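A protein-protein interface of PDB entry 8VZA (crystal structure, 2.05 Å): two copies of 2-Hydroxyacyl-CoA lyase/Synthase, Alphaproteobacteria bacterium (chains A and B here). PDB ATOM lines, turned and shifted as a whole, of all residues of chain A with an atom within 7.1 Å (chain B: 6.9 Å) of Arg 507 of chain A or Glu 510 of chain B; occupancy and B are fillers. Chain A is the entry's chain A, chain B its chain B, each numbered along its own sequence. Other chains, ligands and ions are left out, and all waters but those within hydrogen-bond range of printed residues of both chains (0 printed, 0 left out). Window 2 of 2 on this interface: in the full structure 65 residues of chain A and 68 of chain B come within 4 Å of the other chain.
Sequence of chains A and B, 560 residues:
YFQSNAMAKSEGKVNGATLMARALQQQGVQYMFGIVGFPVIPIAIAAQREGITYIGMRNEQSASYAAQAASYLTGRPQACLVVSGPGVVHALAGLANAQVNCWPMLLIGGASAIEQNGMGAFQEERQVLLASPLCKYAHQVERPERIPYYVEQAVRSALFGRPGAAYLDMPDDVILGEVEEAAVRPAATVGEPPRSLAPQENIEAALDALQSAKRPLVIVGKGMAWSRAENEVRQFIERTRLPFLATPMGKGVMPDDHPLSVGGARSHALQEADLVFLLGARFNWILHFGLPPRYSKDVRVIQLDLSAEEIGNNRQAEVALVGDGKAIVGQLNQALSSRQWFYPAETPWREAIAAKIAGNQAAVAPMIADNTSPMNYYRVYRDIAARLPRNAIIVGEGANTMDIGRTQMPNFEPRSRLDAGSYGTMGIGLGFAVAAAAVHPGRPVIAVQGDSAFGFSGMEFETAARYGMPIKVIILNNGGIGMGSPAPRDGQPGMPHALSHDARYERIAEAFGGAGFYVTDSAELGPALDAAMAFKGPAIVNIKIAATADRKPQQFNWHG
The backbone carbonyl oxygen (O) of Glu 510 of chain B lies within hydrogen-bond range of the guanidinium group (NH1) of Arg 507 of chain A (3.0 Å). The backbone NH of Arg 504 of chain B is in hydrogen-bond range of the backbone carbonyl oxygen of Ala 511 of chain A, at 2.8 Å. The backbone NH of Arg 504 of chain A is in hydrogen-bond range of the backbone carbonyl oxygen of Ala 511 of chain B. The backbone carbonyl oxygen of Glu 510 of chain A lies within hydrogen-bond range of the guanidinium group of Arg 507 of chain B (2.9 Å).
The side-chain carboxylate (OE2) of Glu 506 of chain A lies within salt-bridge range of the guanidinium group (NE) of Arg 504 of chain A. The backbone carbonyl oxygen of Ala 503 of chain A sits at hydrogen-bond distance from the side-chain amide nitrogen of Asn 542 of chain A (2.8 Å). NE of Arg 504 of chain B is in salt-bridge range of OE2 of Glu 506 of chain B (3.0 Å). The side-chain amide nitrogen (ND2) of Asn 542 of chain A sits close to the backbone NH (N) of Tyr 505 of chain A, at 3.0 Å.
Among the printed residues, pairs that only touch across the chains: Ala 503 of chain A with Ala 511 of chain B (3.8 Å), Ala 503 of chain A with Phe 512 of chain B (3.8 Å), Tyr 505 of chain A with Phe 512 of chain B (3.3 Å), Arg 507 of chain A with Ala 511 of chain B (3.95 Å), Ala 511 of chain A with Arg 507 of chain B (3.97 Å), Phe 512 of chain A with Tyr 505 of chain B (3.5 Å) and Phe 512 of chain A with Ile 508 of chain B (3.97 Å).
Printed residues of chain B within 4 Å of Ala 503 of chain A: Ala 511 (3.8 Å) and Phe 512 (3.8 Å). Of the printed residues of chain B, Arg 504 of chain A touches Ala 511. Arg 507 of chain A touches just these residues of chain B: Glu 510 and Ala 511. Printed residues of chain B within 4 Å of Glu 510 of chain A: Arg 507. Phe 461 of chain B touches none of the printed residues of chain A. Of the printed residues of chain A, Tyr 505 of chain B touches Phe 512 (3.5 Å). Glu 510 of chain B touches just one residue of chain A: Arg 507. Ala 515 of chain B touches none of the printed residues of chain A. The nearest residue of chain B that does not touch Arg 507 of chain A is Arg 507 of chain B (4.1 Å).
Printed residues of chain A that touch a printed residue of chain B: Ala 503, Arg 504, Tyr 505, Arg 507, Glu 510, Ala 511 and Phe 512. Hydrophobic or aromatic side chains of chain A within 4 Å of the printed part of chain B: Ala 503, Tyr 505, Ala 511 and Phe 512. Of the 16 printed residues of chain B, 7 touch a printed residue of chain A. Along chain B the printed residues that touch a printed residue of chain A span positions 504 to 512. Among the printed residues, 11 pairs touch across the chains.
Arg 504 of chain A touches Ala 511 of chain B, and with the chains exchanged Ala 511 of chain A touches Arg 504 of chain B. Tyr 505 of chain A touches Phe 512 of chain B, and with the chains exchanged Phe 512 of chain A touches Tyr 505 of chain B. Arg 507 of chain A touches Glu 510 of chain B, and with the chains exchanged Glu 510 of chain A touches Arg 507 of chain B. Phe 512 of chain A touches Ile 508 of chain B, but with the chains exchanged Ile 508 of chain A does not touch Phe 512 of chain B (4.3 Å). Positions printed for both chains: 504, 505, 506, 507, 508, 509, 510, 511, 512, 514, 516, 517 and 540. Of the 11 pairs that touch across the chains among the printed residues, 8 have their exchanged pair printed and touching as well.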
ATOM      1  N   ALA A 503     -16.838  -7.355   4.094  1.00  0.00           N
ATOM      2  CA  ALA A 503     -16.328  -8.625   3.592  1.00  0.00           C
ATOM      3  C   ALA A 503     -17.415  -9.694   3.589  1.00  0.00           C
ATOM      4  O   ALA A 503     -18.229  -9.783   4.511  1.00  0.00           O
ATOM      5  CB  ALA A 503     -15.145  -9.092   4.439  1.00  0.00           C
ATOM      6  N   ARG A 504     -17.418 -10.516   2.544  1.00  0.00           N
ATOM      7  CA  ARG A 504     -18.366 -11.621   2.426  1.00  0.00           C
ATOM      8  C   ARG A 504     -17.650 -12.936   2.731  1.00  0.00           C
ATOM      9  O   ARG A 504     -17.403 -13.775   1.864  1.00  0.00           O
ATOM     10  CB  ARG A 504     -19.001 -11.627   1.038  1.00  0.00           C
ATOM     11  CG  ARG A 504     -19.646 -10.311   0.650  1.00  0.00           C
ATOM     12  CD  ARG A 504     -20.896 -10.045   1.472  1.00  0.00           C
ATOM     13  NE  ARG A 504     -21.960 -10.976   1.124  1.00  0.00           N
ATOM     14  CZ  ARG A 504     -22.913 -10.726   0.237  1.00  0.00           C
ATOM     15  NH1 ARG A 504     -22.988  -9.562  -0.390  1.00  0.00           N
ATOM     16  NH2 ARG A 504     -23.814 -11.667  -0.028  1.00  0.00           N
ATOM     17  N   TYR A 505     -17.326 -13.099   4.016  1.00  0.00           N
ATOM     18  CA  TYR A 505     -16.593 -14.276   4.466  1.00  0.00           C
ATOM     19  C   TYR A 505     -17.339 -15.567   4.158  1.00  0.00           C
ATOM     20  O   TYR A 505     -16.711 -16.616   3.982  1.00  0.00           O
ATOM     21  CB  TYR A 505     -16.324 -14.183   5.969  1.00  0.00           C
ATOM     22  CG  TYR A 505     -15.323 -13.128   6.387  1.00  0.00           C
ATOM     23  CD1 TYR A 505     -13.973 -13.262   6.085  1.00  0.00           C
ATOM     24  CD2 TYR A 505     -15.722 -12.012   7.113  1.00  0.00           C
ATOM     25  CE1 TYR A 505     -13.046 -12.304   6.481  1.00  0.00           C
ATOM     26  CE2 TYR A 505     -14.808 -11.049   7.513  1.00  0.00           C
ATOM     27  CZ  TYR A 505     -13.472 -11.200   7.190  1.00  0.00           C
ATOM     28  OH  TYR A 505     -12.558 -10.248   7.586  1.00  0.00           O
ATOM     29  N   GLU A 506     -18.669 -15.517   4.088  1.00  0.00           N
ATOM     30  CA  GLU A 506     -19.429 -16.731   3.825  1.00  0.00           C
ATOM     31  C   GLU A 506     -19.167 -17.301   2.433  1.00  0.00           C
ATOM     32  O   GLU A 506     -19.381 -18.498   2.225  1.00  0.00           O
ATOM     33  CB  GLU A 506     -20.926 -16.472   4.024  1.00  0.00           C
ATOM     34  CG  GLU A 506     -21.615 -15.735   2.885  1.00  0.00           C
ATOM     35  CD  GLU A 506     -21.238 -14.267   2.801  1.00  0.00           C
ATOM     36  OE1 GLU A 506     -20.529 -13.769   3.703  1.00  0.00           O
ATOM     37  OE2 GLU A 506     -21.653 -13.604   1.825  1.00  0.00           O
ATOM     38  N   ARG A 507     -18.698 -16.488   1.479  1.00  0.00           N
ATOM     39  CA  ARG A 507     -18.365 -17.022   0.160  1.00  0.00           C
ATOM     40  C   ARG A 507     -17.201 -18.007   0.205  1.00  0.00           C
ATOM     41  O   ARG A 507     -17.071 -18.831  -0.705  1.00  0.00           O
ATOM     42  CB  ARG A 507     -18.040 -15.893  -0.821  1.00  0.00           C
ATOM     43  CG  ARG A 507     -19.164 -14.890  -1.006  1.00  0.00           C
ATOM     44  CD  ARG A 507     -18.913 -13.981  -2.201  1.00  0.00           C
ATOM     45  NE  ARG A 507     -19.843 -12.858  -2.235  1.00  0.00           N
ATOM     46  CZ  ARG A 507     -19.928 -11.978  -3.225  1.00  0.00           C
ATOM     47  NH1 ARG A 507     -19.175 -12.081  -4.308  1.00  0.00           N
ATOM     48  NH2 ARG A 507     -20.793 -10.974  -3.126  1.00  0.00           N
ATOM     49  N   ILE A 508     -16.351 -17.936   1.229  1.00  0.00           N
ATOM     50  CA  ILE A 508     -15.297 -18.936   1.380  1.00  0.00           C
ATOM     51  C   ILE A 508     -15.898 -20.335   1.459  1.00  0.00           C
ATOM     52  O   ILE A 508     -15.362 -21.291   0.887  1.00  0.00           O
ATOM     53  CB  ILE A 508     -14.431 -18.610   2.613  1.00  0.00           C
ATOM     54  CG1 ILE A 508     -13.728 -17.263   2.419  1.00  0.00           C
ATOM     55  CG2 ILE A 508     -13.408 -19.709   2.868  1.00  0.00           C
ATOM     56  CD1 ILE A 508     -13.118 -16.707   3.682  1.00  0.00           C
ATOM     57  N   ALA A 509     -17.036 -20.471   2.148  1.00  0.00           N
ATOM     58  CA  ALA A 509     -17.701 -21.766   2.245  1.00  0.00           C
ATOM     59  C   ALA A 509     -18.121 -22.280   0.874  1.00  0.00           C
ATOM     60  O   ALA A 509     -18.035 -23.482   0.601  1.00  0.00           O
ATOM     61  CB  ALA A 509     -18.916 -21.666   3.167  1.00  0.00           C
ATOM     62  N   GLU A 510     -18.587 -21.385   0.002  1.00  0.00           N
ATOM     63  CA  GLU A 510     -19.001 -21.804  -1.331  1.00  0.00           C
ATOM     64  C   GLU A 510     -17.812 -22.176  -2.200  1.00  0.00           C
ATOM     65  O   GLU A 510     -17.994 -22.796  -3.252  1.00  0.00           O
ATOM     66  CB  GLU A 510     -19.822 -20.704  -2.003  1.00  0.00           C
ATOM     67  CG  GLU A 510     -21.129 -20.386  -1.279  1.00  0.00           C
ATOM     68  CD  GLU A 510     -21.742 -19.060  -1.714  1.00  0.00           C
ATOM     69  OE1 GLU A 510     -21.207 -18.425  -2.650  1.00  0.00           O
ATOM     70  OE2 GLU A 510     -22.758 -18.649  -1.109  1.00  0.00           O
ATOM     71  N   ALA A 511     -16.601 -21.814  -1.784  1.00  0.00           N
ATOM     72  CA  ALA A 511     -15.423 -22.236  -2.526  1.00  0.00           C
ATOM     73  C   ALA A 511     -15.106 -23.708  -2.303  1.00  0.00           C
ATOM     74  O   ALA A 511     -14.455 -24.325  -3.152  1.00  0.00           O
ATOM     75  CB  ALA A 511     -14.221 -21.373  -2.137  1.00  0.00           C
ATOM     76  N   PHE A 512     -15.572 -24.290  -1.195  1.00  0.00           N
ATOM     77  CA  PHE A 512     -15.198 -25.646  -0.811  1.00  0.00           C
ATOM     78  C   PHE A 512     -16.405 -26.560  -0.629  1.00  0.00           C
ATOM     79  O   PHE A 512     -16.283 -27.618  -0.009  1.00  0.00           O
ATOM     80  CB  PHE A 512     -14.354 -25.616   0.465  1.00  0.00           C
ATOM     81  CG  PHE A 512     -13.157 -24.715   0.370  1.00  0.00           C
ATOM     82  CD1 PHE A 512     -12.179 -24.944  -0.588  1.00  0.00           C
ATOM     83  CD2 PHE A 512     -13.011 -23.638   1.220  1.00  0.00           C
ATOM     84  CE1 PHE A 512     -11.074 -24.113  -0.680  1.00  0.00           C
ATOM     85  CE2 PHE A 512     -11.911 -22.806   1.130  1.00  0.00           C
ATOM     86  CZ  PHE A 512     -10.943 -23.044   0.182  1.00  0.00           C
ATOM     87  N   GLY A 514     -19.273 -26.030   1.042  1.00  0.00           N
ATOM     88  CA  GLY A 514     -20.133 -25.759   2.174  1.00  0.00           C
ATOM     89  C   GLY A 514     -21.219 -24.747   1.853  1.00  0.00           C
ATOM     90  O   GLY A 514     -21.322 -24.216   0.746  1.00  0.00           O
ATOM     91  N   GLY A 516     -22.910 -21.114   2.595  1.00  0.00           N
ATOM     92  CA  GLY A 516     -22.617 -19.771   3.073  1.00  0.00           C
ATOM     93  C   GLY A 516     -23.896 -18.965   3.215  1.00  0.00           C
ATOM     94  O   GLY A 516     -24.796 -19.062   2.378  1.00  0.00           O
ATOM     95  N   PHE A 517     -23.968 -18.178   4.282  1.00  0.00           N
ATOM     96  CA  PHE A 517     -25.106 -17.314   4.551  1.00  0.00           C
ATOM     97  C   PHE A 517     -24.599 -15.944   4.972  1.00  0.00           C
ATOM     98  O   PHE A 517     -23.600 -15.839   5.689  1.00  0.00           O
ATOM     99  CB  PHE A 517     -26.013 -17.895   5.652  1.00  0.00           C
ATOM    100  CG  PHE A 517     -26.451 -19.312   5.403  1.00  0.00           C
ATOM    101  CD1 PHE A 517     -25.685 -20.380   5.853  1.00  0.00           C
ATOM    102  CD2 PHE A 517     -27.632 -19.576   4.729  1.00  0.00           C
ATOM    103  CE1 PHE A 517     -26.088 -21.684   5.627  1.00  0.00           C
ATOM    104  CE2 PHE A 517     -28.043 -20.879   4.501  1.00  0.00           C
ATOM    105  CZ  PHE A 517     -27.270 -21.933   4.950  1.00  0.00           C
ATOM    106  N   ILE A 540     -20.838 -21.498   6.968  1.00  0.00           N
ATOM    107  CA  ILE A 540     -20.391 -20.219   7.501  1.00  0.00           C
ATOM    108  C   ILE A 540     -21.587 -19.277   7.539  1.00  0.00           C
ATOM    109  O   ILE A 540     -22.268 -19.093   6.526  1.00  0.00           O
ATOM    110  CB  ILE A 540     -19.257 -19.603   6.658  1.00  0.00           C
ATOM    111  CG1 ILE A 540     -17.982 -20.446   6.758  1.00  0.00           C
ATOM    112  CG2 ILE A 540     -18.984 -18.187   7.113  1.00  0.00           C
ATOM    113  CD1 ILE A 540     -16.857 -19.968   5.861  1.00  0.00           C
ATOM    114  N   ASN A 542     -22.064 -15.384   8.149  1.00  0.00           N
ATOM    115  CA  ASN A 542     -21.365 -14.107   8.235  1.00  0.00           C
ATOM    116  C   ASN A 542     -22.359 -13.035   8.674  1.00  0.00           C
ATOM    117  O   ASN A 542     -23.309 -12.734   7.947  1.00  0.00           O
ATOM    118  CB  ASN A 542     -20.744 -13.752   6.881  1.00  0.00           C
ATOM    119  CG  ASN A 542     -19.879 -12.505   6.931  1.00  0.00           C
ATOM    120  OD1 ASN A 542     -19.490 -12.038   8.004  1.00  0.00           O
ATOM    121  ND2 ASN A 542     -19.557 -11.969   5.760  1.00  0.00           N
ATOM    122  N   PHE B 461      -5.227 -12.705   1.085  1.00  0.00           N
ATOM    123  CA  PHE B 461      -5.864 -12.007  -0.024  1.00  0.00           C
ATOM    124  C   PHE B 461      -6.733 -10.853   0.475  1.00  0.00           C
ATOM    125  O   PHE B 461      -6.823  -9.816  -0.195  1.00  0.00           O
ATOM    126  CB  PHE B 461      -6.687 -12.992  -0.862  1.00  0.00           C
ATOM    127  CG  PHE B 461      -7.093 -12.451  -2.208  1.00  0.00           C
ATOM    128  CD1 PHE B 461      -8.276 -11.742  -2.357  1.00  0.00           C
ATOM    129  CD2 PHE B 461      -6.293 -12.650  -3.322  1.00  0.00           C
ATOM    130  CE1 PHE B 461      -8.647 -11.238  -3.593  1.00  0.00           C
ATOM    131  CE2 PHE B 461      -6.655 -12.151  -4.559  1.00  0.00           C
ATOM    132  CZ  PHE B 461      -7.836 -11.451  -4.699  1.00  0.00           C
ATOM    133  N   ARG B 504     -13.093 -24.451  -5.588  1.00  0.00           N
ATOM    134  CA  ARG B 504     -13.229 -23.205  -6.349  1.00  0.00           C
ATOM    135  C   ARG B 504     -12.559 -22.063  -5.589  1.00  0.00           C
ATOM    136  O   ARG B 504     -13.204 -21.154  -5.063  1.00  0.00           O
ATOM    137  CB  ARG B 504     -14.698 -22.912  -6.627  1.00  0.00           C
ATOM    138  CG  ARG B 504     -15.434 -24.065  -7.295  1.00  0.00           C
ATOM    139  CD  ARG B 504     -15.040 -24.202  -8.759  1.00  0.00           C
ATOM    140  NE  ARG B 504     -15.293 -22.974  -9.505  1.00  0.00           N
ATOM    141  CZ  ARG B 504     -16.333 -22.772 -10.303  1.00  0.00           C
ATOM    142  NH1 ARG B 504     -17.253 -23.703 -10.494  1.00  0.00           N
ATOM    143  NH2 ARG B 504     -16.450 -21.605 -10.929  1.00  0.00           N
ATOM    144  N   TYR B 505     -11.221 -22.133  -5.554  1.00  0.00           N
ATOM    145  CA  TYR B 505     -10.435 -21.171  -4.785  1.00  0.00           C
ATOM    146  C   TYR B 505     -10.665 -19.732  -5.241  1.00  0.00           C
ATOM    147  O   TYR B 505     -10.543 -18.801  -4.435  1.00  0.00           O
ATOM    148  CB  TYR B 505      -8.946 -21.509  -4.884  1.00  0.00           C
ATOM    149  CG  TYR B 505      -8.516 -22.775  -4.170  1.00  0.00           C
ATOM    150  CD1 TYR B 505      -8.351 -22.802  -2.790  1.00  0.00           C
ATOM    151  CD2 TYR B 505      -8.247 -23.936  -4.881  1.00  0.00           C
ATOM    152  CE1 TYR B 505      -7.945 -23.960  -2.140  1.00  0.00           C
ATOM    153  CE2 TYR B 505      -7.839 -25.088  -4.244  1.00  0.00           C
ATOM    154  CZ  TYR B 505      -7.692 -25.100  -2.875  1.00  0.00           C
ATOM    155  OH  TYR B 505      -7.286 -26.265  -2.258  1.00  0.00           O
ATOM    156  N   GLU B 506     -10.988 -19.520  -6.520  1.00  0.00           N
ATOM    157  CA  GLU B 506     -11.161 -18.153  -7.002  1.00  0.00           C
ATOM    158  C   GLU B 506     -12.349 -17.452  -6.346  1.00  0.00           C
ATOM    159  O   GLU B 506     -12.412 -16.219  -6.365  1.00  0.00           O
ATOM    160  CB  GLU B 506     -11.313 -18.137  -8.525  1.00  0.00           C
ATOM    161  CG  GLU B 506     -12.722 -18.432  -9.034  1.00  0.00           C
ATOM    162  CD  GLU B 506     -13.107 -19.899  -8.919  1.00  0.00           C
ATOM    163  OE1 GLU B 506     -12.215 -20.734  -8.664  1.00  0.00           O
ATOM    164  OE2 GLU B 506     -14.308 -20.216  -9.087  1.00  0.00           O
ATOM    165  N   ARG B 507     -13.281 -18.203  -5.755  1.00  0.00           N
ATOM    166  CA  ARG B 507     -14.387 -17.579  -5.041  1.00  0.00           C
ATOM    167  C   ARG B 507     -13.938 -16.873  -3.767  1.00  0.00           C
ATOM    168  O   ARG B 507     -14.724 -16.114  -3.191  1.00  0.00           O
ATOM    169  CB  ARG B 507     -15.458 -18.622  -4.718  1.00  0.00           C
ATOM    170  CG  ARG B 507     -16.037 -19.298  -5.954  1.00  0.00           C
ATOM    171  CD  ARG B 507     -17.389 -19.916  -5.665  1.00  0.00           C
ATOM    172  NE  ARG B 507     -18.035 -20.428  -6.869  1.00  0.00           N
ATOM    173  CZ  ARG B 507     -18.395 -21.692  -7.050  1.00  0.00           C
ATOM    174  NH1 ARG B 507     -18.181 -22.610  -6.122  1.00  0.00           N
ATOM    175  NH2 ARG B 507     -18.998 -22.042  -8.184  1.00  0.00           N
ATOM    176  N   ILE B 508     -12.704 -17.105  -3.317  1.00  0.00           N
ATOM    177  CA  ILE B 508     -12.178 -16.376  -2.169  1.00  0.00           C
ATOM    178  C   ILE B 508     -11.913 -14.922  -2.540  1.00  0.00           C
ATOM    179  O   ILE B 508     -12.098 -14.013  -1.721  1.00  0.00           O
ATOM    180  CB  ILE B 508     -10.910 -17.072  -1.642  1.00  0.00           C
ATOM    181  CG1 ILE B 508     -11.232 -18.511  -1.221  1.00  0.00           C
ATOM    182  CG2 ILE B 508     -10.305 -16.288  -0.482  1.00  0.00           C
ATOM    183  CD1 ILE B 508     -10.003 -19.357  -0.947  1.00  0.00           C
ATOM    184  N   ALA B 509     -11.482 -14.679  -3.782  1.00  0.00           N
ATOM    185  CA  ALA B 509     -11.308 -13.310  -4.252  1.00  0.00           C
ATOM    186  C   ALA B 509     -12.621 -12.539  -4.188  1.00  0.00           C
ATOM    187  O   ALA B 509     -12.666 -11.399  -3.711  1.00  0.00           O
ATOM    188  CB  ALA B 509     -10.752 -13.309  -5.677  1.00  0.00           C
ATOM    189  N   GLU B 510     -13.704 -13.161  -4.658  1.00  0.00           N
ATOM    190  CA  GLU B 510     -15.011 -12.515  -4.676  1.00  0.00           C
ATOM    191  C   GLU B 510     -15.536 -12.230  -3.273  1.00  0.00           C
ATOM    192  O   GLU B 510     -16.464 -11.430  -3.121  1.00  0.00           O
ATOM    193  CB  GLU B 510     -16.003 -13.388  -5.454  1.00  0.00           C
ATOM    194  CG  GLU B 510     -15.537 -13.720  -6.874  1.00  0.00           C
ATOM    195  CD  GLU B 510     -16.350 -14.827  -7.541  1.00  0.00           C
ATOM    196  OE1 GLU B 510     -17.458 -15.142  -7.058  1.00  0.00           O
ATOM    197  OE2 GLU B 510     -15.871 -15.388  -8.552  1.00  0.00           O
ATOM    198  N   ALA B 511     -14.965 -12.861  -2.247  1.00  0.00           N
ATOM    199  CA  ALA B 511     -15.354 -12.569  -0.875  1.00  0.00           C
ATOM    200  C   ALA B 511     -14.807 -11.237  -0.382  1.00  0.00           C
ATOM    201  O   ALA B 511     -15.361 -10.668   0.565  1.00  0.00           O
ATOM    202  CB  ALA B 511     -14.883 -13.685   0.061  1.00  0.00           C
ATOM    203  N   PHE B 512     -13.737 -10.727  -0.999  1.00  0.00           N
ATOM    204  CA  PHE B 512     -13.100  -9.491  -0.557  1.00  0.00           C
ATOM    205  C   PHE B 512     -13.005  -8.456  -1.673  1.00  0.00           C
ATOM    206  O   PHE B 512     -12.158  -7.558  -1.610  1.00  0.00           O
ATOM    207  CB  PHE B 512     -11.710  -9.777   0.014  1.00  0.00           C
ATOM    208  CG  PHE B 512     -11.703 -10.809   1.105  1.00  0.00           C
ATOM    209  CD1 PHE B 512     -12.393 -10.590   2.285  1.00  0.00           C
ATOM    210  CD2 PHE B 512     -11.000 -11.994   0.950  1.00  0.00           C
ATOM    211  CE1 PHE B 512     -12.391 -11.540   3.295  1.00  0.00           C
ATOM    212  CE2 PHE B 512     -10.988 -12.950   1.957  1.00  0.00           C
ATOM    213  CZ  PHE B 512     -11.686 -12.721   3.132  1.00  0.00           C
ATOM    214  N   GLY B 513     -13.850  -8.563  -2.698  1.00  0.00           N
ATOM    215  CA  GLY B 513     -13.910  -7.562  -3.740  1.00  0.00           C
ATOM    216  C   GLY B 513     -12.977  -7.781  -4.910  1.00  0.00           C
ATOM    217  O   GLY B 513     -13.096  -7.068  -5.915  1.00  0.00           O
ATOM    218  N   GLY B 514     -12.052  -8.732  -4.818  1.00  0.00           N
ATOM    219  CA  GLY B 514     -11.191  -9.055  -5.934  1.00  0.00           C
ATOM    220  C   GLY B 514     -11.956  -9.713  -7.071  1.00  0.00           C
ATOM    221  O   GLY B 514     -13.180  -9.850  -7.056  1.00  0.00           O
ATOM    222  N   ALA B 515     -11.200 -10.133  -8.081  1.00  0.00           N
ATOM    223  CA  ALA B 515     -11.748 -10.787  -9.261  1.00  0.00           C
ATOM    224  C   ALA B 515     -11.338 -12.252  -9.259  1.00  0.00           C
ATOM    225  O   ALA B 515     -10.169 -12.570  -9.024  1.00  0.00           O
ATOM    226  CB  ALA B 515     -11.262 -10.107 -10.542  1.00  0.00           C
ATOM    227  N   GLY B 516     -12.300 -13.136  -9.519  1.00  0.00           N
ATOM    228  CA  GLY B 516     -12.033 -14.559  -9.540  1.00  0.00           C
ATOM    229  C   GLY B 516     -12.288 -15.202 -10.888  1.00  0.00           C
ATOM    230  O   GLY B 516     -13.308 -14.935 -11.528  1.00  0.00           O
ATOM    231  N   PHE B 517     -11.364 -16.054 -11.329  1.00  0.00           N
ATOM    232  CA  PHE B 517     -11.451 -16.718 -12.622  1.00  0.00           C
ATOM    233  C   PHE B 517     -11.187 -18.201 -12.426  1.00  0.00           C
ATOM    234  O   PHE B 517     -10.261 -18.580 -11.701  1.00  0.00           O
ATOM    235  CB  PHE B 517     -10.455 -16.115 -13.625  1.00  0.00           C
ATOM    236  CG  PHE B 517     -10.668 -14.651 -13.871  1.00  0.00           C
ATOM    237  CD1 PHE B 517     -11.559 -14.220 -14.838  1.00  0.00           C
ATOM    238  CD2 PHE B 517      -9.997 -13.702 -13.113  1.00  0.00           C
ATOM    239  CE1 PHE B 517     -11.774 -12.870 -15.057  1.00  0.00           C
ATOM    240  CE2 PHE B 517     -10.203 -12.351 -13.328  1.00  0.00           C
ATOM    241  CZ  PHE B 517     -11.094 -11.934 -14.298  1.00  0.00           C
ATOM    242  N   ILE B 540      -7.511 -13.766  -8.373  1.00  0.00           N
ATOM    243  CA  ILE B 540      -7.133 -15.171  -8.278  1.00  0.00           C
ATOM    244  C   ILE B 540      -7.588 -15.871  -9.547  1.00  0.00           C
ATOM    245  O   ILE B 540      -8.763 -15.786  -9.920  1.00  0.00           O
ATOM    246  CB  ILE B 540      -7.754 -15.862  -7.051  1.00  0.00           C
ATOM    247  CG1 ILE B 540      -7.203 -15.292  -5.753  1.00  0.00           C
ATOM    248  CG2 ILE B 540      -7.502 -17.361  -7.102  1.00  0.00           C
ATOM    249  CD1 ILE B 540      -7.906 -15.833  -4.543  1.00  0.00           C
